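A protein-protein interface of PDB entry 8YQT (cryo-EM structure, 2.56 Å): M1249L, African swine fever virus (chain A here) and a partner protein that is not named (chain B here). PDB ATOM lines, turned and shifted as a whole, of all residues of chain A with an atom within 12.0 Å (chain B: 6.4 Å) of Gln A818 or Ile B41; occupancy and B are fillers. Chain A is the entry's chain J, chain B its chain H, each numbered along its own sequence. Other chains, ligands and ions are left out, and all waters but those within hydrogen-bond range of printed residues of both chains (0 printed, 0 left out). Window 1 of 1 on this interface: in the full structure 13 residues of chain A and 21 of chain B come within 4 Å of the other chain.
The side-chain amino group (NZ) of Lys B78 lies within salt-bridge range of the side-chain carboxylate (OD1) of Asp B22 (3.3 Å). The backbone carbonyl oxygen (O) of Ala A814 lies close to the side-chain amide nitrogen (NE2) of Gln A818, at 3.2 Å.
Among the printed residues, merely in contact across the chains: Glu A811 with Pro B38 (3.0 Å), Gln A818 with Pro B42 (3.2 Å), Asn A823 with Ala B45 (3.3 Å), Leu A815 with Pro B38 (3.4 Å), Gln A818 with Ile B29 (3.4 Å), Ala A817 with Lys B78 (3.6 Å), Leu A815 with Met B33 (3.6 Å), Tyr A822 with Leu B47 (3.7 Å), Phe A821 with Ile B41 (3.7 Å), Leu A816 with Thr B26 (3.7 Å), Leu A815 with Thr B26 (3.7 Å), Lys A813 with Lys B78 (3.7 Å), Phe A821 with Pro B42 (3.8 Å), Gln A818 with Ile B41 (3.8 Å), Ala A814 with Pro B38 (3.8 Å), Phe A821 with Leu B47 (3.8 Å), Gly A820 with Ile B29 (3.9 Å) and Tyr A822 with Ile B49 (3.95 Å).
NH2 of Arg B25 lies within hydrogen-bond range of O of Gln A819 (3.2 Å). O of Pro B38 is in hydrogen-bond range of NE2 of Gln A818. The side-chain amide oxygen (OE1) of Gln B39 sits close to the side-chain carboxylate (OE1) of Glu A811 (2.6 Å). The backbone carbonyl oxygen (O) of Leu B47 is in hydrogen-bond range of the side-chain amide nitrogen (ND2) of Asn A823 (3.0 Å). N of Ile B49 lies within hydrogen-bond range of O of Phe A821, at 3.1 Å. O of Leu A816 sits at hydrogen-bond distance from NZ of Lys B78, 3.3 Å away.
Of the 18 printed residues of chain B, 12 touch a printed residue of chain A. Hydrophobic or aromatic side chains of chain B within 4 Å of the printed part of chain A: Ile B29, Met B33, Pro B38, Ile B41, Pro B42, Leu B47 and Ile B49. Printed residues of chain A that touch a printed residue of chain B: Glu A811, Lys A813, Ala A814, Leu A815, Leu A816, Ala A817, Gln A818, Gln A819, Gly A820, Phe A821, Tyr A822 and Asn A823. Among the printed residues, 24 pairs touch across the chains. Among the printed residues, no Asp or Glu carboxylate lies within 4 Å of a Lys or Arg side-chain nitrogen of the other chain.
Of chain B, only Ile B29, Pro B38, Ile B41 and Pro B42 come within 4 Å of Gln A818. Ile B41 touches just these residues of chain A: Gln A818 and Phe A821. Arg B25 touches just one residue of chain A: Gln A819 (3.2 Å). Ile B29 touches two residues of chain A. Printed residues of chain A within 4 Å of Met B33: Leu A815. No residue of chain A comes within 4 Å of Thr B36. Pro B38 touches just these residues of chain A: Glu A811, Ala A814, Leu A815 and Gln A818. Of chain A, only Glu A811 comes within 4 Å of Gln B39. Pro B42 touches just these residues of chain A: Gln A818 (3.2 Å) and Phe A821 (3.8 Å). Asp B44 touches none of the printed residues of chain A. Of the printed residues of chain B, Phe A821 touches Ile B41 (3.7 Å), Pro B42 (3.8 Å), Leu B47 (3.8 Å) and Ile B49 (3.1 Å). Of the printed residues of chain B, Lys A813 touches Lys B78. Of the printed residues of chain B, Tyr A822 touches Leu B47 (3.7 Å) and Ile B49 (3.95 Å). Ile A824 touches none of the printed residues of chain B. Asp B22 touches none of the printed residues of chain A. The nearest residue of chain B that does not touch Gln A818 is Gln B39 (4.03 Å). The nearest residue of chain A that does not touch Ile B41 is Leu A815 (4.3 Å). The nearest printed residue of chain B that does not touch Gln A819 is Ile B29 (4.2 Å).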
ATOM      1  N   TYR A 809     -30.658  22.367  35.819  1.00  0.00           N
ATOM      2  CA  TYR A 809     -29.239  22.577  36.085  1.00  0.00           C
ATOM      3  C   TYR A 809     -28.362  21.839  35.078  1.00  0.00           C
ATOM      4  O   TYR A 809     -27.340  22.371  34.631  1.00  0.00           O
ATOM      5  CB  TYR A 809     -28.918  22.132  37.510  1.00  0.00           C
ATOM      6  CG  TYR A 809     -27.493  22.373  37.940  1.00  0.00           C
ATOM      7  CD1 TYR A 809     -26.993  23.660  38.060  1.00  0.00           C
ATOM      8  CD2 TYR A 809     -26.654  21.312  38.246  1.00  0.00           C
ATOM      9  CE1 TYR A 809     -25.694  23.884  38.460  1.00  0.00           C
ATOM     10  CE2 TYR A 809     -25.354  21.526  38.646  1.00  0.00           C
ATOM     11  CZ  TYR A 809     -24.878  22.813  38.753  1.00  0.00           C
ATOM     12  OH  TYR A 809     -23.581  23.029  39.153  1.00  0.00           O
ATOM     13  N   GLY A 810     -28.745  20.615  34.710  1.00  0.00           N
ATOM     14  CA  GLY A 810     -28.015  19.883  33.695  1.00  0.00           C
ATOM     15  C   GLY A 810     -28.155  20.491  32.318  1.00  0.00           C
ATOM     16  O   GLY A 810     -27.252  20.365  31.492  1.00  0.00           O
ATOM     17  N   GLU A 811     -29.281  21.151  32.049  1.00  0.00           N
ATOM     18  CA  GLU A 811     -29.393  21.934  30.823  1.00  0.00           C
ATOM     19  C   GLU A 811     -28.347  23.043  30.791  1.00  0.00           C
ATOM     20  O   GLU A 811     -27.661  23.242  29.776  1.00  0.00           O
ATOM     21  CB  GLU A 811     -30.801  22.515  30.705  1.00  0.00           C
ATOM     22  CG  GLU A 811     -31.198  22.886  29.297  1.00  0.00           C
ATOM     23  CD  GLU A 811     -31.101  21.711  28.352  1.00  0.00           C
ATOM     24  OE1 GLU A 811     -30.202  21.725  27.491  1.00  0.00           O
ATOM     25  OE2 GLU A 811     -31.920  20.776  28.470  1.00  0.00           O
ATOM     26  N   GLN A 812     -28.190  23.757  31.908  1.00  0.00           N
ATOM     27  CA  GLN A 812     -27.131  24.764  31.990  1.00  0.00           C
ATOM     28  C   GLN A 812     -25.754  24.136  31.787  1.00  0.00           C
ATOM     29  O   GLN A 812     -24.927  24.647  31.020  1.00  0.00           O
ATOM     30  CB  GLN A 812     -27.181  25.495  33.334  1.00  0.00           C
ATOM     31  CG  GLN A 812     -28.555  25.620  33.947  1.00  0.00           C
ATOM     32  CD  GLN A 812     -29.198  26.960  33.675  1.00  0.00           C
ATOM     33  OE1 GLN A 812     -28.650  27.788  32.948  1.00  0.00           O
ATOM     34  NE2 GLN A 812     -30.370  27.181  34.257  1.00  0.00           N
ATOM     35  N   LYS A 813     -25.491  23.020  32.472  1.00  0.00           N
ATOM     36  CA  LYS A 813     -24.187  22.372  32.374  1.00  0.00           C
ATOM     37  C   LYS A 813     -23.901  21.838  30.977  1.00  0.00           C
ATOM     38  O   LYS A 813     -22.736  21.794  30.571  1.00  0.00           O
ATOM     39  CB  LYS A 813     -24.079  21.235  33.389  1.00  0.00           C
ATOM     40  CG  LYS A 813     -23.459  21.646  34.714  1.00  0.00           C
ATOM     41  CD  LYS A 813     -22.726  20.489  35.380  1.00  0.00           C
ATOM     42  CE  LYS A 813     -22.179  19.498  34.356  1.00  0.00           C
ATOM     43  NZ  LYS A 813     -21.125  18.623  34.934  1.00  0.00           N
ATOM     44  N   ALA A 814     -24.931  21.418  30.244  1.00  0.00           N
ATOM     45  CA  ALA A 814     -24.769  21.041  28.849  1.00  0.00           C
ATOM     46  C   ALA A 814     -24.520  22.246  27.963  1.00  0.00           C
ATOM     47  O   ALA A 814     -23.850  22.115  26.934  1.00  0.00           O
ATOM     48  CB  ALA A 814     -26.004  20.288  28.355  1.00  0.00           C
ATOM     49  N   LEU A 815     -25.059  23.411  28.327  1.00  0.00           N
ATOM     50  CA  LEU A 815     -24.673  24.632  27.629  1.00  0.00           C
ATOM     51  C   LEU A 815     -23.196  24.934  27.843  1.00  0.00           C
ATOM     52  O   LEU A 815     -22.495  25.332  26.906  1.00  0.00           O
ATOM     53  CB  LEU A 815     -25.544  25.804  28.087  1.00  0.00           C
ATOM     54  CG  LEU A 815     -25.389  27.172  27.409  1.00  0.00           C
ATOM     55  CD1 LEU A 815     -24.346  28.029  28.107  1.00  0.00           C
ATOM     56  CD2 LEU A 815     -25.069  27.034  25.925  1.00  0.00           C
ATOM     57  N   LEU A 816     -22.705  24.748  29.071  1.00  0.00           N
ATOM     58  CA  LEU A 816     -21.297  25.022  29.347  1.00  0.00           C
ATOM     59  C   LEU A 816     -20.370  24.050  28.628  1.00  0.00           C
ATOM     60  O   LEU A 816     -19.210  24.385  28.368  1.00  0.00           O
ATOM     61  CB  LEU A 816     -21.030  24.973  30.849  1.00  0.00           C
ATOM     62  CG  LEU A 816     -21.488  26.184  31.655  1.00  0.00           C
ATOM     63  CD1 LEU A 816     -21.156  25.992  33.124  1.00  0.00           C
ATOM     64  CD2 LEU A 816     -20.845  27.445  31.115  1.00  0.00           C
ATOM     65  N   ALA A 817     -20.853  22.857  28.297  1.00  0.00           N
ATOM     66  CA  ALA A 817     -20.029  21.815  27.703  1.00  0.00           C
ATOM     67  C   ALA A 817     -19.987  21.879  26.183  1.00  0.00           C
ATOM     68  O   ALA A 817     -19.370  21.011  25.559  1.00  0.00           O
ATOM     69  CB  ALA A 817     -20.525  20.438  28.144  1.00  0.00           C
ATOM     70  N   GLN A 818     -20.621  22.874  25.572  1.00  0.00           N
ATOM     71  CA  GLN A 818     -20.684  22.961  24.122  1.00  0.00           C
ATOM     72  C   GLN A 818     -19.413  23.583  23.562  1.00  0.00           C
ATOM     73  O   GLN A 818     -18.925  24.598  24.066  1.00  0.00           O
ATOM     74  CB  GLN A 818     -21.904  23.770  23.682  1.00  0.00           C
ATOM     75  CG  GLN A 818     -23.213  23.043  23.906  1.00  0.00           C
ATOM     76  CD  GLN A 818     -23.216  21.666  23.279  1.00  0.00           C
ATOM     77  OE1 GLN A 818     -22.823  21.495  22.127  1.00  0.00           O
ATOM     78  NE2 GLN A 818     -23.648  20.670  24.042  1.00  0.00           N
ATOM     79  N   GLN A 819     -18.883  22.964  22.510  1.00  0.00           N
ATOM     80  CA  GLN A 819     -17.645  23.401  21.889  1.00  0.00           C
ATOM     81  C   GLN A 819     -17.851  24.091  20.550  1.00  0.00           C
ATOM     82  O   GLN A 819     -16.869  24.523  19.939  1.00  0.00           O
ATOM     83  CB  GLN A 819     -16.700  22.207  21.706  1.00  0.00           C
ATOM     84  CG  GLN A 819     -15.984  21.799  22.979  1.00  0.00           C
ATOM     85  CD  GLN A 819     -15.092  20.599  22.783  1.00  0.00           C
ATOM     86  OE1 GLN A 819     -15.165  19.916  21.764  1.00  0.00           O
ATOM     87  NE2 GLN A 819     -14.236  20.337  23.759  1.00  0.00           N
ATOM     88  N   GLY A 820     -19.083  24.209  20.084  1.00  0.00           N
ATOM     89  CA  GLY A 820     -19.382  24.859  18.829  1.00  0.00           C
ATOM     90  C   GLY A 820     -19.749  23.859  17.745  1.00  0.00           C
ATOM     91  O   GLY A 820     -19.449  22.665  17.824  1.00  0.00           O
ATOM     92  N   PHE A 821     -20.418  24.369  16.718  1.00  0.00           N
ATOM     93  CA  PHE A 821     -20.796  23.554  15.575  1.00  0.00           C
ATOM     94  C   PHE A 821     -20.944  24.461  14.365  1.00  0.00           C
ATOM     95  O   PHE A 821     -21.354  25.617  14.488  1.00  0.00           O
ATOM     96  CB  PHE A 821     -22.089  22.777  15.840  1.00  0.00           C
ATOM     97  CG  PHE A 821     -22.491  21.875  14.714  1.00  0.00           C
ATOM     98  CD1 PHE A 821     -21.670  20.835  14.319  1.00  0.00           C
ATOM     99  CD2 PHE A 821     -23.690  22.064  14.051  1.00  0.00           C
ATOM    100  CE1 PHE A 821     -22.035  20.006  13.284  1.00  0.00           C
ATOM    101  CE2 PHE A 821     -24.059  21.236  13.014  1.00  0.00           C
ATOM    102  CZ  PHE A 821     -23.231  20.207  12.630  1.00  0.00           C
ATOM    103  N   TYR A 822     -20.599  23.925  13.199  1.00  0.00           N
ATOM    104  CA  TYR A 822     -20.593  24.699  11.969  1.00  0.00           C
ATOM    105  C   TYR A 822     -21.204  23.882  10.844  1.00  0.00           C
ATOM    106  O   TYR A 822     -21.050  22.660  10.785  1.00  0.00           O
ATOM    107  CB  TYR A 822     -19.174  25.130  11.591  1.00  0.00           C
ATOM    108  CG  TYR A 822     -19.076  25.968  10.339  1.00  0.00           C
ATOM    109  CD1 TYR A 822     -19.279  27.338  10.379  1.00  0.00           C
ATOM    110  CD2 TYR A 822     -18.769  25.389   9.117  1.00  0.00           C
ATOM    111  CE1 TYR A 822     -19.186  28.104   9.239  1.00  0.00           C
ATOM    112  CE2 TYR A 822     -18.677  26.145   7.974  1.00  0.00           C
ATOM    113  CZ  TYR A 822     -18.886  27.502   8.039  1.00  0.00           C
ATOM    114  OH  TYR A 822     -18.794  28.260   6.897  1.00  0.00           O
ATOM    115  N   ASN A 823     -21.900  24.579   9.951  1.00  0.00           N
ATOM    116  CA  ASN A 823     -22.519  23.982   8.775  1.00  0.00           C
ATOM    117  C   ASN A 823     -22.042  24.746   7.553  1.00  0.00           C
ATOM    118  O   ASN A 823     -22.203  25.969   7.487  1.00  0.00           O
ATOM    119  CB  ASN A 823     -24.044  24.035   8.870  1.00  0.00           C
ATOM    120  CG  ASN A 823     -24.589  23.120   9.933  1.00  0.00           C
ATOM    121  OD1 ASN A 823     -24.711  21.916   9.727  1.00  0.00           O
ATOM    122  ND2 ASN A 823     -24.895  23.683  11.092  1.00  0.00           N
ATOM    123  N   ILE A 824     -21.459  24.036   6.593  1.00  0.00           N
ATOM    124  CA  ILE A 824     -21.066  24.675   5.345  1.00  0.00           C
ATOM    125  C   ILE A 824     -22.322  24.949   4.532  1.00  0.00           C
ATOM    126  O   ILE A 824     -23.050  24.023   4.156  1.00  0.00           O
ATOM    127  CB  ILE A 824     -20.073  23.804   4.567  1.00  0.00           C
ATOM    128  CG1 ILE A 824     -18.866  23.463   5.440  1.00  0.00           C
ATOM    129  CG2 ILE A 824     -19.622  24.515   3.307  1.00  0.00           C
ATOM    130  CD1 ILE A 824     -18.020  22.341   4.896  1.00  0.00           C
ATOM    131  N   PHE A 825     -22.590  26.221   4.269  1.00  0.00           N
ATOM    132  CA  PHE A 825     -23.782  26.614   3.536  1.00  0.00           C
ATOM    133  C   PHE A 825     -23.489  26.708   2.047  1.00  0.00           C
ATOM    134  O   PHE A 825     -22.401  27.107   1.629  1.00  0.00           O
ATOM    135  CB  PHE A 825     -24.319  27.958   4.034  1.00  0.00           C
ATOM    136  CG  PHE A 825     -25.049  27.881   5.345  1.00  0.00           C
ATOM    137  CD1 PHE A 825     -25.191  26.677   6.011  1.00  0.00           C
ATOM    138  CD2 PHE A 825     -25.603  29.016   5.905  1.00  0.00           C
ATOM    139  CE1 PHE A 825     -25.863  26.611   7.212  1.00  0.00           C
ATOM    140  CE2 PHE A 825     -26.276  28.954   7.103  1.00  0.00           C
ATOM    141  CZ  PHE A 825     -26.406  27.751   7.757  1.00  0.00           C
ATOM    142  N   ALA A 832     -27.763  24.375   4.875  1.00  0.00           N
ATOM    143  CA  ALA A 832     -26.727  23.358   4.740  1.00  0.00           C
ATOM    144  C   ALA A 832     -26.576  22.914   3.291  1.00  0.00           C
ATOM    145  O   ALA A 832     -27.561  22.715   2.576  1.00  0.00           O
ATOM    146  CB  ALA A 832     -27.045  22.157   5.629  1.00  0.00           C
ATOM    147  N   ASP B  22     -11.890  29.331  27.195  1.00  0.00           N
ATOM    148  CA  ASP B  22     -13.070  28.547  27.519  1.00  0.00           C
ATOM    149  C   ASP B  22     -14.264  29.454  27.761  1.00  0.00           C
ATOM    150  O   ASP B  22     -15.295  29.339  27.086  1.00  0.00           O
ATOM    151  CB  ASP B  22     -12.795  27.675  28.739  1.00  0.00           C
ATOM    152  CG  ASP B  22     -13.837  26.599  28.927  1.00  0.00           C
ATOM    153  OD1 ASP B  22     -14.235  25.969  27.924  1.00  0.00           O
ATOM    154  OD2 ASP B  22     -14.258  26.384  30.083  1.00  0.00           O
ATOM    155  N   ARG B  25     -15.699  31.369  24.928  1.00  0.00           N
ATOM    156  CA  ARG B  25     -16.485  30.497  24.059  1.00  0.00           C
ATOM    157  C   ARG B  25     -17.938  30.501  24.469  1.00  0.00           C
ATOM    158  O   ARG B  25     -18.823  30.775  23.648  1.00  0.00           O
ATOM    159  CB  ARG B  25     -15.988  29.059  24.113  1.00  0.00           C
ATOM    160  CG  ARG B  25     -14.758  28.735  23.358  1.00  0.00           C
ATOM    161  CD  ARG B  25     -14.337  27.349  23.778  1.00  0.00           C
ATOM    162  NE  ARG B  25     -14.516  26.368  22.718  1.00  0.00           N
ATOM    163  CZ  ARG B  25     -14.130  25.105  22.810  1.00  0.00           C
ATOM    164  NH1 ARG B  25     -13.601  24.626  23.924  1.00  0.00           N
ATOM    165  NH2 ARG B  25     -14.259  24.310  21.754  1.00  0.00           N
ATOM    166  N   THR B  26     -18.196  30.254  25.754  1.00  0.00           N
ATOM    167  CA  THR B  26     -19.572  30.159  26.209  1.00  0.00           C
ATOM    168  C   THR B  26     -20.333  31.416  25.836  1.00  0.00           C
ATOM    169  O   THR B  26     -21.388  31.342  25.192  1.00  0.00           O
ATOM    170  CB  THR B  26     -19.608  29.917  27.714  1.00  0.00           C
ATOM    171  OG1 THR B  26     -18.787  28.787  28.031  1.00  0.00           O
ATOM    172  CG2 THR B  26     -21.021  29.647  28.170  1.00  0.00           C
ATOM    173  N   ILE B  29     -21.018  31.482  22.216  1.00  0.00           N
ATOM    174  CA  ILE B  29     -22.053  30.526  21.851  1.00  0.00           C
ATOM    175  C   ILE B  29     -23.412  31.015  22.326  1.00  0.00           C
ATOM    176  O   ILE B  29     -24.411  30.889  21.604  1.00  0.00           O
ATOM    177  CB  ILE B  29     -21.702  29.130  22.397  1.00  0.00           C
ATOM    178  CG1 ILE B  29     -20.523  28.554  21.613  1.00  0.00           C
ATOM    179  CG2 ILE B  29     -22.894  28.197  22.306  1.00  0.00           C
ATOM    180  CD1 ILE B  29     -19.931  27.311  22.218  1.00  0.00           C
ATOM    181  N   MET B  33     -26.694  30.662  19.737  1.00  0.00           N
ATOM    182  CA  MET B  33     -27.419  29.403  19.875  1.00  0.00           C
ATOM    183  C   MET B  33     -28.906  29.526  19.570  1.00  0.00           C
ATOM    184  O   MET B  33     -29.515  28.541  19.137  1.00  0.00           O
ATOM    185  CB  MET B  33     -27.232  28.834  21.282  1.00  0.00           C
ATOM    186  CG  MET B  33     -27.751  29.719  22.395  1.00  0.00           C
ATOM    187  SD  MET B  33     -27.484  28.981  24.012  1.00  0.00           S
ATOM    188  CE  MET B  33     -28.439  27.479  23.848  1.00  0.00           C
ATOM    189  N   THR B  36     -32.563  26.875  20.218  1.00  0.00           N
ATOM    190  CA  THR B  36     -32.211  25.466  20.307  1.00  0.00           C
ATOM    191  C   THR B  36     -31.694  25.135  21.701  1.00  0.00           C
ATOM    192  O   THR B  36     -30.968  25.922  22.313  1.00  0.00           O
ATOM    193  CB  THR B  36     -31.154  25.124  19.254  1.00  0.00           C
ATOM    194  OG1 THR B  36     -31.646  25.473  17.956  1.00  0.00           O
ATOM    195  CG2 THR B  36     -30.819  23.643  19.270  1.00  0.00           C
ATOM    196  N   LEU B  37     -32.081  23.968  22.207  1.00  0.00           N
ATOM    197  CA  LEU B  37     -31.568  23.514  23.486  1.00  0.00           C
ATOM    198  C   LEU B  37     -30.066  23.259  23.382  1.00  0.00           C
ATOM    199  O   LEU B  37     -29.560  22.905  22.314  1.00  0.00           O
ATOM    200  CB  LEU B  37     -32.282  22.242  23.937  1.00  0.00           C
ATOM    201  CG  LEU B  37     -33.714  22.385  24.453  1.00  0.00           C
ATOM    202  CD1 LEU B  37     -34.280  21.026  24.821  1.00  0.00           C
ATOM    203  CD2 LEU B  37     -33.773  23.330  25.637  1.00  0.00           C
ATOM    204  N   PRO B  38     -29.329  23.456  24.478  1.00  0.00           N
ATOM    205  CA  PRO B  38     -27.870  23.259  24.432  1.00  0.00           C
ATOM    206  C   PRO B  38     -27.423  21.915  23.881  1.00  0.00           C
ATOM    207  O   PRO B  38     -26.566  21.884  22.991  1.00  0.00           O
ATOM    208  CB  PRO B  38     -27.474  23.429  25.901  1.00  0.00           C
ATOM    209  CG  PRO B  38     -28.447  24.423  26.411  1.00  0.00           C
ATOM    210  CD  PRO B  38     -29.747  24.154  25.705  1.00  0.00           C
ATOM    211  N   GLN B  39     -27.981  20.803  24.365  1.00  0.00           N
ATOM    212  CA  GLN B  39     -27.498  19.497  23.925  1.00  0.00           C
ATOM    213  C   GLN B  39     -27.807  19.213  22.462  1.00  0.00           C
ATOM    214  O   GLN B  39     -27.251  18.261  21.907  1.00  0.00           O
ATOM    215  CB  GLN B  39     -28.081  18.380  24.793  1.00  0.00           C
ATOM    216  CG  GLN B  39     -29.521  18.018  24.490  1.00  0.00           C
ATOM    217  CD  GLN B  39     -30.480  18.524  25.540  1.00  0.00           C
ATOM    218  OE1 GLN B  39     -30.125  19.365  26.358  1.00  0.00           O
ATOM    219  NE2 GLN B  39     -31.700  18.005  25.530  1.00  0.00           N
ATOM    220  N   ASN B  40     -28.674  20.000  21.833  1.00  0.00           N
ATOM    221  CA  ASN B  40     -28.968  19.867  20.415  1.00  0.00           C
ATOM    222  C   ASN B  40     -28.171  20.844  19.562  1.00  0.00           C
ATOM    223  O   ASN B  40     -28.395  20.918  18.352  1.00  0.00           O
ATOM    224  CB  ASN B  40     -30.464  20.058  20.168  1.00  0.00           C
ATOM    225  CG  ASN B  40     -31.316  19.162  21.042  1.00  0.00           C
ATOM    226  OD1 ASN B  40     -30.880  18.096  21.468  1.00  0.00           O
ATOM    227  ND2 ASN B  40     -32.536  19.599  21.322  1.00  0.00           N
ATOM    228  N   ILE B  41     -27.255  21.605  20.174  1.00  0.00           N
ATOM    229  CA  ILE B  41     -26.435  22.543  19.400  1.00  0.00           C
ATOM    230  C   ILE B  41     -25.635  21.840  18.314  1.00  0.00           C
ATOM    231  O   ILE B  41     -25.578  22.357  17.189  1.00  0.00           O
ATOM    232  CB  ILE B  41     -25.571  23.391  20.344  1.00  0.00           C
ATOM    233  CG1 ILE B  41     -26.389  24.547  20.917  1.00  0.00           C
ATOM    234  CG2 ILE B  41     -24.341  23.924  19.631  1.00  0.00           C
ATOM    235  CD1 ILE B  41     -25.656  25.350  21.961  1.00  0.00           C
ATOM    236  N   PRO B  42     -25.006  20.674  18.548  1.00  0.00           N
ATOM    237  CA  PRO B  42     -24.309  19.997  17.445  1.00  0.00           C
ATOM    238  C   PRO B  42     -25.242  19.318  16.452  1.00  0.00           C
ATOM    239  O   PRO B  42     -24.792  18.522  15.623  1.00  0.00           O
ATOM    240  CB  PRO B  42     -23.428  18.970  18.165  1.00  0.00           C
ATOM    241  CG  PRO B  42     -24.058  18.780  19.479  1.00  0.00           C
ATOM    242  CD  PRO B  42     -24.634  20.093  19.850  1.00  0.00           C
ATOM    243  N   LEU B  43     -26.539  19.622  16.523  1.00  0.00           N
ATOM    244  CA  LEU B  43     -27.523  19.061  15.606  1.00  0.00           C
ATOM    245  C   LEU B  43     -28.333  20.127  14.878  1.00  0.00           C
ATOM    246  O   LEU B  43     -29.234  19.776  14.108  1.00  0.00           O
ATOM    247  CB  LEU B  43     -28.482  18.129  16.355  1.00  0.00           C
ATOM    248  CG  LEU B  43     -28.005  16.734  16.747  1.00  0.00           C
ATOM    249  CD1 LEU B  43     -28.824  16.216  17.910  1.00  0.00           C
ATOM    250  CD2 LEU B  43     -28.110  15.796  15.560  1.00  0.00           C
ATOM    251  N   ASP B  44     -28.039  21.412  15.091  1.00  0.00           N
ATOM    252  CA  ASP B  44     -28.943  22.468  14.647  1.00  0.00           C
ATOM    253  C   ASP B  44     -29.052  22.543  13.127  1.00  0.00           C
ATOM    254  O   ASP B  44     -30.137  22.814  12.600  1.00  0.00           O
ATOM    255  CB  ASP B  44     -28.503  23.815  15.217  1.00  0.00           C
ATOM    256  CG  ASP B  44     -29.590  24.874  15.121  1.00  0.00           C
ATOM    257  OD1 ASP B  44     -30.678  24.573  14.593  1.00  0.00           O
ATOM    258  OD2 ASP B  44     -29.363  26.011  15.580  1.00  0.00           O
ATOM    259  N   ALA B  45     -27.951  22.323  12.413  1.00  0.00           N
ATOM    260  CA  ALA B  45     -27.887  22.380  10.954  1.00  0.00           C
ATOM    261  C   ALA B  45     -28.139  23.778  10.404  1.00  0.00           C
ATOM    262  O   ALA B  45     -28.255  23.951   9.186  1.00  0.00           O
ATOM    263  CB  ALA B  45     -28.853  21.386  10.301  1.00  0.00           C
ATOM    264  N   LEU B  47     -26.483  26.464  12.486  1.00  0.00           N
ATOM    265  CA  LEU B  47     -25.460  27.209  13.198  1.00  0.00           C
ATOM    266  C   LEU B  47     -24.192  27.314  12.366  1.00  0.00           C
ATOM    267  O   LEU B  47     -23.823  26.382  11.647  1.00  0.00           O
ATOM    268  CB  LEU B  47     -25.140  26.540  14.532  1.00  0.00           C
ATOM    269  CG  LEU B  47     -26.216  26.614  15.608  1.00  0.00           C
ATOM    270  CD1 LEU B  47     -25.785  25.843  16.840  1.00  0.00           C
ATOM    271  CD2 LEU B  47     -26.516  28.055  15.951  1.00  0.00           C
ATOM    272  N   ILE B  49     -20.743  28.615  13.820  1.00  0.00           N
ATOM    273  CA  ILE B  49     -20.009  29.154  14.959  1.00  0.00           C
ATOM    274  C   ILE B  49     -18.524  29.070  14.639  1.00  0.00           C
ATOM    275  O   ILE B  49     -17.949  27.978  14.589  1.00  0.00           O
ATOM    276  CB  ILE B  49     -20.353  28.406  16.252  1.00  0.00           C
ATOM    277  CG1 ILE B  49     -21.792  28.711  16.670  1.00  0.00           C
ATOM    278  CG2 ILE B  49     -19.380  28.769  17.356  1.00  0.00           C
ATOM    279  CD1 ILE B  49     -22.333  27.773  17.716  1.00  0.00           C
ATOM    280  N   LYS B  78     -16.805  19.403  32.637  1.00  0.00           N
ATOM    281  CA  LYS B  78     -18.083  19.605  31.973  1.00  0.00           C
ATOM    282  C   LYS B  78     -18.869  18.316  31.780  1.00  0.00           C
ATOM    283  O   LYS B  78     -20.038  18.377  31.390  1.00  0.00           O
ATOM    284  CB  LYS B  78     -17.864  20.274  30.616  1.00  0.00           C
ATOM    285  CG  LYS B  78     -16.816  21.359  30.635  1.00  0.00           C
ATOM    286  CD  LYS B  78     -17.435  22.727  30.782  1.00  0.00           C
ATOM    287  CE  LYS B  78     -16.534  23.789  30.191  1.00  0.00           C
ATOM    288  NZ  LYS B  78     -16.127  23.442  28.805  1.00  0.00           N
